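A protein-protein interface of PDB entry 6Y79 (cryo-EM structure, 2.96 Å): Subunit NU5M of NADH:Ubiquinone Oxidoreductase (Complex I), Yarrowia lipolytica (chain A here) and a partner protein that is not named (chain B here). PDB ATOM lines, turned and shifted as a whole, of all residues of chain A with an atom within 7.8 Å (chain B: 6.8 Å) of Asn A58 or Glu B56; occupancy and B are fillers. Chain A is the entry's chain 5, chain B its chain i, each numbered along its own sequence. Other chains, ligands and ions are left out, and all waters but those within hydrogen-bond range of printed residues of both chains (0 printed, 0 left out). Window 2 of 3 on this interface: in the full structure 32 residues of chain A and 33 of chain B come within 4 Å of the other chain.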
ATOM      1  N   TYR A  49     -18.840 -14.591  -5.535  1.00  0.00           N
ATOM      2  CA  TYR A  49     -19.283 -14.404  -6.912  1.00  0.00           C
ATOM      3  C   TYR A  49     -18.165 -14.691  -7.905  1.00  0.00           C
ATOM      4  O   TYR A  49     -18.421 -15.209  -8.999  1.00  0.00           O
ATOM      5  CB  TYR A  49     -19.818 -12.989  -7.113  1.00  0.00           C
ATOM      6  CG  TYR A  49     -20.348 -12.754  -8.504  1.00  0.00           C
ATOM      7  CD1 TYR A  49     -21.598 -13.218  -8.872  1.00  0.00           C
ATOM      8  CD2 TYR A  49     -19.593 -12.080  -9.453  1.00  0.00           C
ATOM      9  CE1 TYR A  49     -22.083 -13.012 -10.146  1.00  0.00           C
ATOM     10  CE2 TYR A  49     -20.066 -11.881 -10.722  1.00  0.00           C
ATOM     11  CZ  TYR A  49     -21.310 -12.340 -11.063  1.00  0.00           C
ATOM     12  OH  TYR A  49     -21.775 -12.128 -12.334  1.00  0.00           O
ATOM     13  N   GLN A  52     -18.042 -18.338  -8.244  1.00  0.00           N
ATOM     14  CA  GLN A  52     -19.104 -18.884  -9.087  1.00  0.00           C
ATOM     15  C   GLN A  52     -18.842 -18.618 -10.565  1.00  0.00           C
ATOM     16  O   GLN A  52     -19.094 -19.487 -11.405  1.00  0.00           O
ATOM     17  CB  GLN A  52     -20.470 -18.341  -8.672  1.00  0.00           C
ATOM     18  CG  GLN A  52     -20.880 -18.691  -7.255  1.00  0.00           C
ATOM     19  CD  GLN A  52     -21.607 -20.022  -7.132  1.00  0.00           C
ATOM     20  OE1 GLN A  52     -21.295 -20.995  -7.820  1.00  0.00           O
ATOM     21  NE2 GLN A  52     -22.587 -20.068  -6.239  1.00  0.00           N
ATOM     22  N   LEU A  53     -18.328 -17.427 -10.907  1.00  0.00           N
ATOM     23  CA  LEU A  53     -18.040 -17.126 -12.311  1.00  0.00           C
ATOM     24  C   LEU A  53     -16.855 -17.923 -12.833  1.00  0.00           C
ATOM     25  O   LEU A  53     -16.723 -18.091 -14.045  1.00  0.00           O
ATOM     26  CB  LEU A  53     -17.802 -15.622 -12.516  1.00  0.00           C
ATOM     27  CG  LEU A  53     -17.776 -14.974 -13.914  1.00  0.00           C
ATOM     28  CD1 LEU A  53     -18.411 -13.604 -13.862  1.00  0.00           C
ATOM     29  CD2 LEU A  53     -16.373 -14.837 -14.478  1.00  0.00           C
ATOM     30  N   LEU A  54     -16.008 -18.456 -11.954  1.00  0.00           N
ATOM     31  CA  LEU A  54     -15.044 -19.445 -12.428  1.00  0.00           C
ATOM     32  C   LEU A  54     -15.715 -20.740 -12.878  1.00  0.00           C
ATOM     33  O   LEU A  54     -15.141 -21.460 -13.699  1.00  0.00           O
ATOM     34  CB  LEU A  54     -14.007 -19.726 -11.348  1.00  0.00           C
ATOM     35  CG  LEU A  54     -12.946 -18.631 -11.254  1.00  0.00           C
ATOM     36  CD1 LEU A  54     -11.970 -18.929 -10.147  1.00  0.00           C
ATOM     37  CD2 LEU A  54     -12.219 -18.462 -12.577  1.00  0.00           C
ATOM     38  N   GLY A  55     -16.920 -21.033 -12.385  1.00  0.00           N
ATOM     39  CA  GLY A  55     -17.719 -22.145 -12.867  1.00  0.00           C
ATOM     40  C   GLY A  55     -18.186 -21.982 -14.299  1.00  0.00           C
ATOM     41  O   GLY A  55     -17.782 -22.760 -15.166  1.00  0.00           O
ATOM     42  N   ASN A  56     -19.043 -20.999 -14.568  1.00  0.00           N
ATOM     43  CA  ASN A  56     -19.390 -20.630 -15.933  1.00  0.00           C
ATOM     44  C   ASN A  56     -19.050 -19.167 -16.173  1.00  0.00           C
ATOM     45  O   ASN A  56     -19.247 -18.321 -15.301  1.00  0.00           O
ATOM     46  CB  ASN A  56     -20.880 -20.883 -16.256  1.00  0.00           C
ATOM     47  CG  ASN A  56     -21.838 -20.257 -15.249  1.00  0.00           C
ATOM     48  OD1 ASN A  56     -21.437 -19.691 -14.238  1.00  0.00           O
ATOM     49  ND2 ASN A  56     -23.128 -20.364 -15.538  1.00  0.00           N
ATOM     50  N   ASN A  57     -18.551 -18.862 -17.368  1.00  0.00           N
ATOM     51  CA  ASN A  57     -18.327 -17.473 -17.754  1.00  0.00           C
ATOM     52  C   ASN A  57     -19.651 -16.914 -18.267  1.00  0.00           C
ATOM     53  O   ASN A  57     -19.855 -16.685 -19.462  1.00  0.00           O
ATOM     54  CB  ASN A  57     -17.219 -17.376 -18.792  1.00  0.00           C
ATOM     55  CG  ASN A  57     -16.628 -15.991 -18.885  1.00  0.00           C
ATOM     56  OD1 ASN A  57     -17.040 -15.079 -18.177  1.00  0.00           O
ATOM     57  ND2 ASN A  57     -15.657 -15.826 -19.766  1.00  0.00           N
ATOM     58  N   ASN A  58     -20.574 -16.698 -17.331  1.00  0.00           N
ATOM     59  CA  ASN A  58     -21.910 -16.193 -17.639  1.00  0.00           C
ATOM     60  C   ASN A  58     -22.192 -15.038 -16.693  1.00  0.00           C
ATOM     61  O   ASN A  58     -22.668 -15.239 -15.569  1.00  0.00           O
ATOM     62  CB  ASN A  58     -22.971 -17.283 -17.502  1.00  0.00           C
ATOM     63  CG  ASN A  58     -24.254 -16.932 -18.212  1.00  0.00           C
ATOM     64  OD1 ASN A  58     -24.330 -15.923 -18.906  1.00  0.00           O
ATOM     65  ND2 ASN A  58     -25.272 -17.760 -18.042  1.00  0.00           N
ATOM     66  N   PRO A  59     -21.892 -13.815 -17.111  1.00  0.00           N
ATOM     67  CA  PRO A  59     -22.041 -12.663 -16.219  1.00  0.00           C
ATOM     68  C   PRO A  59     -23.495 -12.268 -16.006  1.00  0.00           C
ATOM     69  O   PRO A  59     -24.396 -12.659 -16.746  1.00  0.00           O
ATOM     70  CB  PRO A  59     -21.280 -11.558 -16.957  1.00  0.00           C
ATOM     71  CG  PRO A  59     -20.356 -12.277 -17.851  1.00  0.00           C
ATOM     72  CD  PRO A  59     -21.108 -13.468 -18.305  1.00  0.00           C
ATOM     73  N   ILE A  60     -23.703 -11.460 -14.972  1.00  0.00           N
ATOM     74  CA  ILE A  60     -25.014 -10.935 -14.611  1.00  0.00           C
ATOM     75  C   ILE A  60     -24.987  -9.421 -14.763  1.00  0.00           C
ATOM     76  O   ILE A  60     -24.034  -8.773 -14.330  1.00  0.00           O
ATOM     77  CB  ILE A  60     -25.388 -11.331 -13.168  1.00  0.00           C
ATOM     78  CG1 ILE A  60     -25.320 -12.847 -12.990  1.00  0.00           C
ATOM     79  CG2 ILE A  60     -26.772 -10.847 -12.805  1.00  0.00           C
ATOM     80  CD1 ILE A  60     -25.438 -13.290 -11.556  1.00  0.00           C
ATOM     81  N   ASN A  61     -26.014  -8.856 -15.402  1.00  0.00           N
ATOM     82  CA  ASN A  61     -26.311  -7.434 -15.293  1.00  0.00           C
ATOM     83  C   ASN A  61     -27.676  -7.229 -14.674  1.00  0.00           C
ATOM     84  O   ASN A  61     -28.585  -8.026 -14.862  1.00  0.00           O
ATOM     85  CB  ASN A  61     -26.302  -6.703 -16.637  1.00  0.00           C
ATOM     86  CG  ASN A  61     -26.948  -7.472 -17.730  1.00  0.00           C
ATOM     87  OD1 ASN A  61     -27.440  -8.562 -17.522  1.00  0.00           O
ATOM     88  ND2 ASN A  61     -26.908  -6.923 -18.935  1.00  0.00           N
ATOM     89  N   ILE A  81     -21.174  -7.305 -14.028  1.00  0.00           N
ATOM     90  CA  ILE A  81     -19.872  -7.761 -13.574  1.00  0.00           C
ATOM     91  C   ILE A  81     -19.338  -8.708 -14.647  1.00  0.00           C
ATOM     92  O   ILE A  81     -19.635  -9.902 -14.686  1.00  0.00           O
ATOM     93  CB  ILE A  81     -19.946  -8.396 -12.196  1.00  0.00           C
ATOM     94  CG1 ILE A  81     -20.374  -7.326 -11.201  1.00  0.00           C
ATOM     95  CG2 ILE A  81     -18.596  -8.815 -11.780  1.00  0.00           C
ATOM     96  CD1 ILE A  81     -20.612  -7.827  -9.814  1.00  0.00           C
ATOM     97  N   ASP A  82     -18.515  -8.139 -15.521  1.00  0.00           N
ATOM     98  CA  ASP A  82     -17.612  -8.791 -16.457  1.00  0.00           C
ATOM     99  C   ASP A  82     -16.579  -9.633 -15.694  1.00  0.00           C
ATOM    100  O   ASP A  82     -16.497  -9.617 -14.465  1.00  0.00           O
ATOM    101  CB  ASP A  82     -16.938  -7.691 -17.300  1.00  0.00           C
ATOM    102  CG  ASP A  82     -16.214  -8.201 -18.541  1.00  0.00           C
ATOM    103  OD1 ASP A  82     -16.178  -9.424 -18.774  1.00  0.00           O
ATOM    104  OD2 ASP A  82     -15.651  -7.357 -19.270  1.00  0.00           O
ATOM    105  N   ARG B  53     -30.432 -10.405 -15.664  1.00  0.00           N
ATOM    106  CA  ARG B  53     -30.404 -11.419 -16.700  1.00  0.00           C
ATOM    107  C   ARG B  53     -28.957 -11.819 -16.923  1.00  0.00           C
ATOM    108  O   ARG B  53     -28.033 -11.132 -16.490  1.00  0.00           O
ATOM    109  CB  ARG B  53     -31.048 -10.920 -17.998  1.00  0.00           C
ATOM    110  CG  ARG B  53     -30.268  -9.831 -18.690  1.00  0.00           C
ATOM    111  CD  ARG B  53     -30.902  -9.443 -20.005  1.00  0.00           C
ATOM    112  NE  ARG B  53     -30.222  -8.304 -20.611  1.00  0.00           N
ATOM    113  CZ  ARG B  53     -29.152  -8.404 -21.392  1.00  0.00           C
ATOM    114  NH1 ARG B  53     -28.599  -7.313 -21.898  1.00  0.00           N
ATOM    115  NH2 ARG B  53     -28.639  -9.593 -21.668  1.00  0.00           N
ATOM    116  N   ARG B  54     -28.766 -12.958 -17.570  1.00  0.00           N
ATOM    117  CA  ARG B  54     -27.421 -13.364 -17.930  1.00  0.00           C
ATOM    118  C   ARG B  54     -26.977 -12.656 -19.206  1.00  0.00           C
ATOM    119  O   ARG B  54     -27.771 -12.039 -19.915  1.00  0.00           O
ATOM    120  CB  ARG B  54     -27.357 -14.874 -18.107  1.00  0.00           C
ATOM    121  CG  ARG B  54     -27.740 -15.627 -16.862  1.00  0.00           C
ATOM    122  CD  ARG B  54     -26.668 -15.484 -15.820  1.00  0.00           C
ATOM    123  NE  ARG B  54     -26.997 -16.209 -14.601  1.00  0.00           N
ATOM    124  CZ  ARG B  54     -26.110 -16.524 -13.666  1.00  0.00           C
ATOM    125  NH1 ARG B  54     -24.840 -16.179 -13.815  1.00  0.00           N
ATOM    126  NH2 ARG B  54     -26.493 -17.182 -12.582  1.00  0.00           N
ATOM    127  N   ARG B  55     -25.687 -12.750 -19.501  1.00  0.00           N
ATOM    128  CA  ARG B  55     -25.168 -12.104 -20.699  1.00  0.00           C
ATOM    129  C   ARG B  55     -25.394 -12.948 -21.948  1.00  0.00           C
ATOM    130  O   ARG B  55     -25.832 -12.435 -22.982  1.00  0.00           O
ATOM    131  CB  ARG B  55     -23.678 -11.817 -20.535  1.00  0.00           C
ATOM    132  CG  ARG B  55     -23.077 -11.041 -21.679  1.00  0.00           C
ATOM    133  CD  ARG B  55     -21.648 -10.657 -21.386  1.00  0.00           C
ATOM    134  NE  ARG B  55     -21.096  -9.798 -22.424  1.00  0.00           N
ATOM    135  CZ  ARG B  55     -20.495 -10.249 -23.518  1.00  0.00           C
ATOM    136  NH1 ARG B  55     -20.017  -9.397 -24.412  1.00  0.00           N
ATOM    137  NH2 ARG B  55     -20.369 -11.554 -23.717  1.00  0.00           N
ATOM    138  N   GLU B  56     -25.110 -14.242 -21.851  1.00  0.00           N
ATOM    139  CA  GLU B  56     -25.224 -15.254 -22.896  1.00  0.00           C
ATOM    140  C   GLU B  56     -26.406 -16.167 -22.582  1.00  0.00           C
ATOM    141  O   GLU B  56     -26.671 -16.498 -21.426  1.00  0.00           O
ATOM    142  CB  GLU B  56     -23.931 -16.106 -22.995  1.00  0.00           C
ATOM    143  CG  GLU B  56     -23.983 -17.277 -23.942  1.00  0.00           C
ATOM    144  CD  GLU B  56     -23.889 -16.857 -25.413  1.00  0.00           C
ATOM    145  OE1 GLU B  56     -22.990 -16.045 -25.726  1.00  0.00           O
ATOM    146  OE2 GLU B  56     -24.805 -17.249 -26.152  1.00  0.00           O
ATOM    147  N   GLY B  57     -27.088 -16.625 -23.629  1.00  0.00           N
ATOM    148  CA  GLY B  57     -28.085 -17.659 -23.478  1.00  0.00           C
ATOM    149  C   GLY B  57     -29.481 -17.125 -23.349  1.00  0.00           C
ATOM    150  O   GLY B  57     -30.408 -17.886 -23.045  1.00  0.00           O
ATOM    151  N   ILE B  58     -29.645 -15.829 -23.576  1.00  0.00           N
ATOM    152  CA  ILE B  58     -30.920 -15.147 -23.491  1.00  0.00           C
ATOM    153  C   ILE B  58     -31.764 -15.530 -24.693  1.00  0.00           C
ATOM    154  O   ILE B  58     -32.829 -16.137 -24.543  1.00  0.00           O
ATOM    155  CB  ILE B  58     -30.721 -13.626 -23.427  1.00  0.00           C
ATOM    156  CG1 ILE B  58     -29.915 -13.251 -22.182  1.00  0.00           C
ATOM    157  CG2 ILE B  58     -32.067 -12.930 -23.457  1.00  0.00           C
ATOM    158  CD1 ILE B  58     -30.578 -13.656 -20.913  1.00  0.00           C
ATOM    159  N   THR B  59     -31.294 -15.193 -25.893  1.00  0.00           N
ATOM    160  CA  THR B  59     -32.059 -15.431 -27.106  1.00  0.00           C
ATOM    161  C   THR B  59     -31.480 -16.621 -27.861  1.00  0.00           C
ATOM    162  O   THR B  59     -30.301 -16.956 -27.695  1.00  0.00           O
ATOM    163  CB  THR B  59     -32.084 -14.182 -28.000  1.00  0.00           C
ATOM    164  OG1 THR B  59     -30.770 -13.889 -28.478  1.00  0.00           O
ATOM    165  CG2 THR B  59     -32.593 -12.994 -27.213  1.00  0.00           C
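OD1 of Asn A58 sits at hydrogen-bond distance from N of Glu B56, 3.5 Å away.
The backbone carbonyl oxygen of Arg B53 sits close to the side-chain amide oxygen of Asn A61, at 2.8 Å.
The guanidinium group (NH1) of Arg B54 lies within hydrogen-bond range of the backbone carbonyl oxygen (O) of Asn A58, 2.9 Å away.
The backbone NH of Arg B55 is in hydrogen-bond range of the backbone carbonyl oxygen of Pro A59 (3.0 Å).
The backbone NH of Ile A81 lies within hydrogen-bond range of the backbone carbonyl oxygen of Ile A60, at 3.2 Å.
OH of Tyr A49 is in hydrogen-bond range of N of Ile A60, at 3.3 Å.
Among the printed residues, merely in contact across the chains: Asn A58 with Arg B55, Pro A59 with Arg B53, Pro A59 with Arg B54, Ile A60 with Arg B53 and Ile A60 with Arg B54.
Leu A54 touches none of the printed residues of chain B.
Asn A57 touches none of the printed residues of chain B.
Of chain B, only Arg B54 (2.9 Å), Arg B55 (3.5 Å) and Glu B56 (3.5 Å) come within 4 Å of Asn A58.
Of the printed residues of chain B, Pro A59 touches Arg B53 (3.95 Å), Arg B54 (3.3 Å) and Arg B55 (3.0 Å).
Of the printed residues of chain B, Ile A60 touches Arg B53 and Arg B54.
Printed residues of chain B within 4 Å of Asn A61: Arg B53 (2.8 Å).
Of the printed residues of chain A, Arg B53 touches Pro A59 (3.95 Å), Ile A60 (3.6 Å) and Asn A61 (2.8 Å).
Printed residues of chain A within 4 Å of Arg B54: Asn A58 (2.9 Å), Pro A59 (3.3 Å) and Ile A60 (3.5 Å).
Of chain A, only Asn A58 comes within 4 Å of Glu B56.
The nearest residue of chain B that does not touch Asn A58 is Gly B57 (5.5 Å).
The nearest residue of chain A that does not touch Glu B56 is Pro A59 (5.4 Å).
Hydrophobic or aromatic side chains of chain A that line the printed part of chain B: Pro A59 and Ile A60.
Along chain A the printed residues that touch a printed residue of chain B span positions 58 to 61.
Of the 7 printed residues of chain B, 4 touch a printed residue of chain A.
Printed residues of chain B that touch a printed residue of chain A: Arg B53, Arg B54, Arg B55 and Glu B56.
Among the printed residues, 9 pairs touch across the chains.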
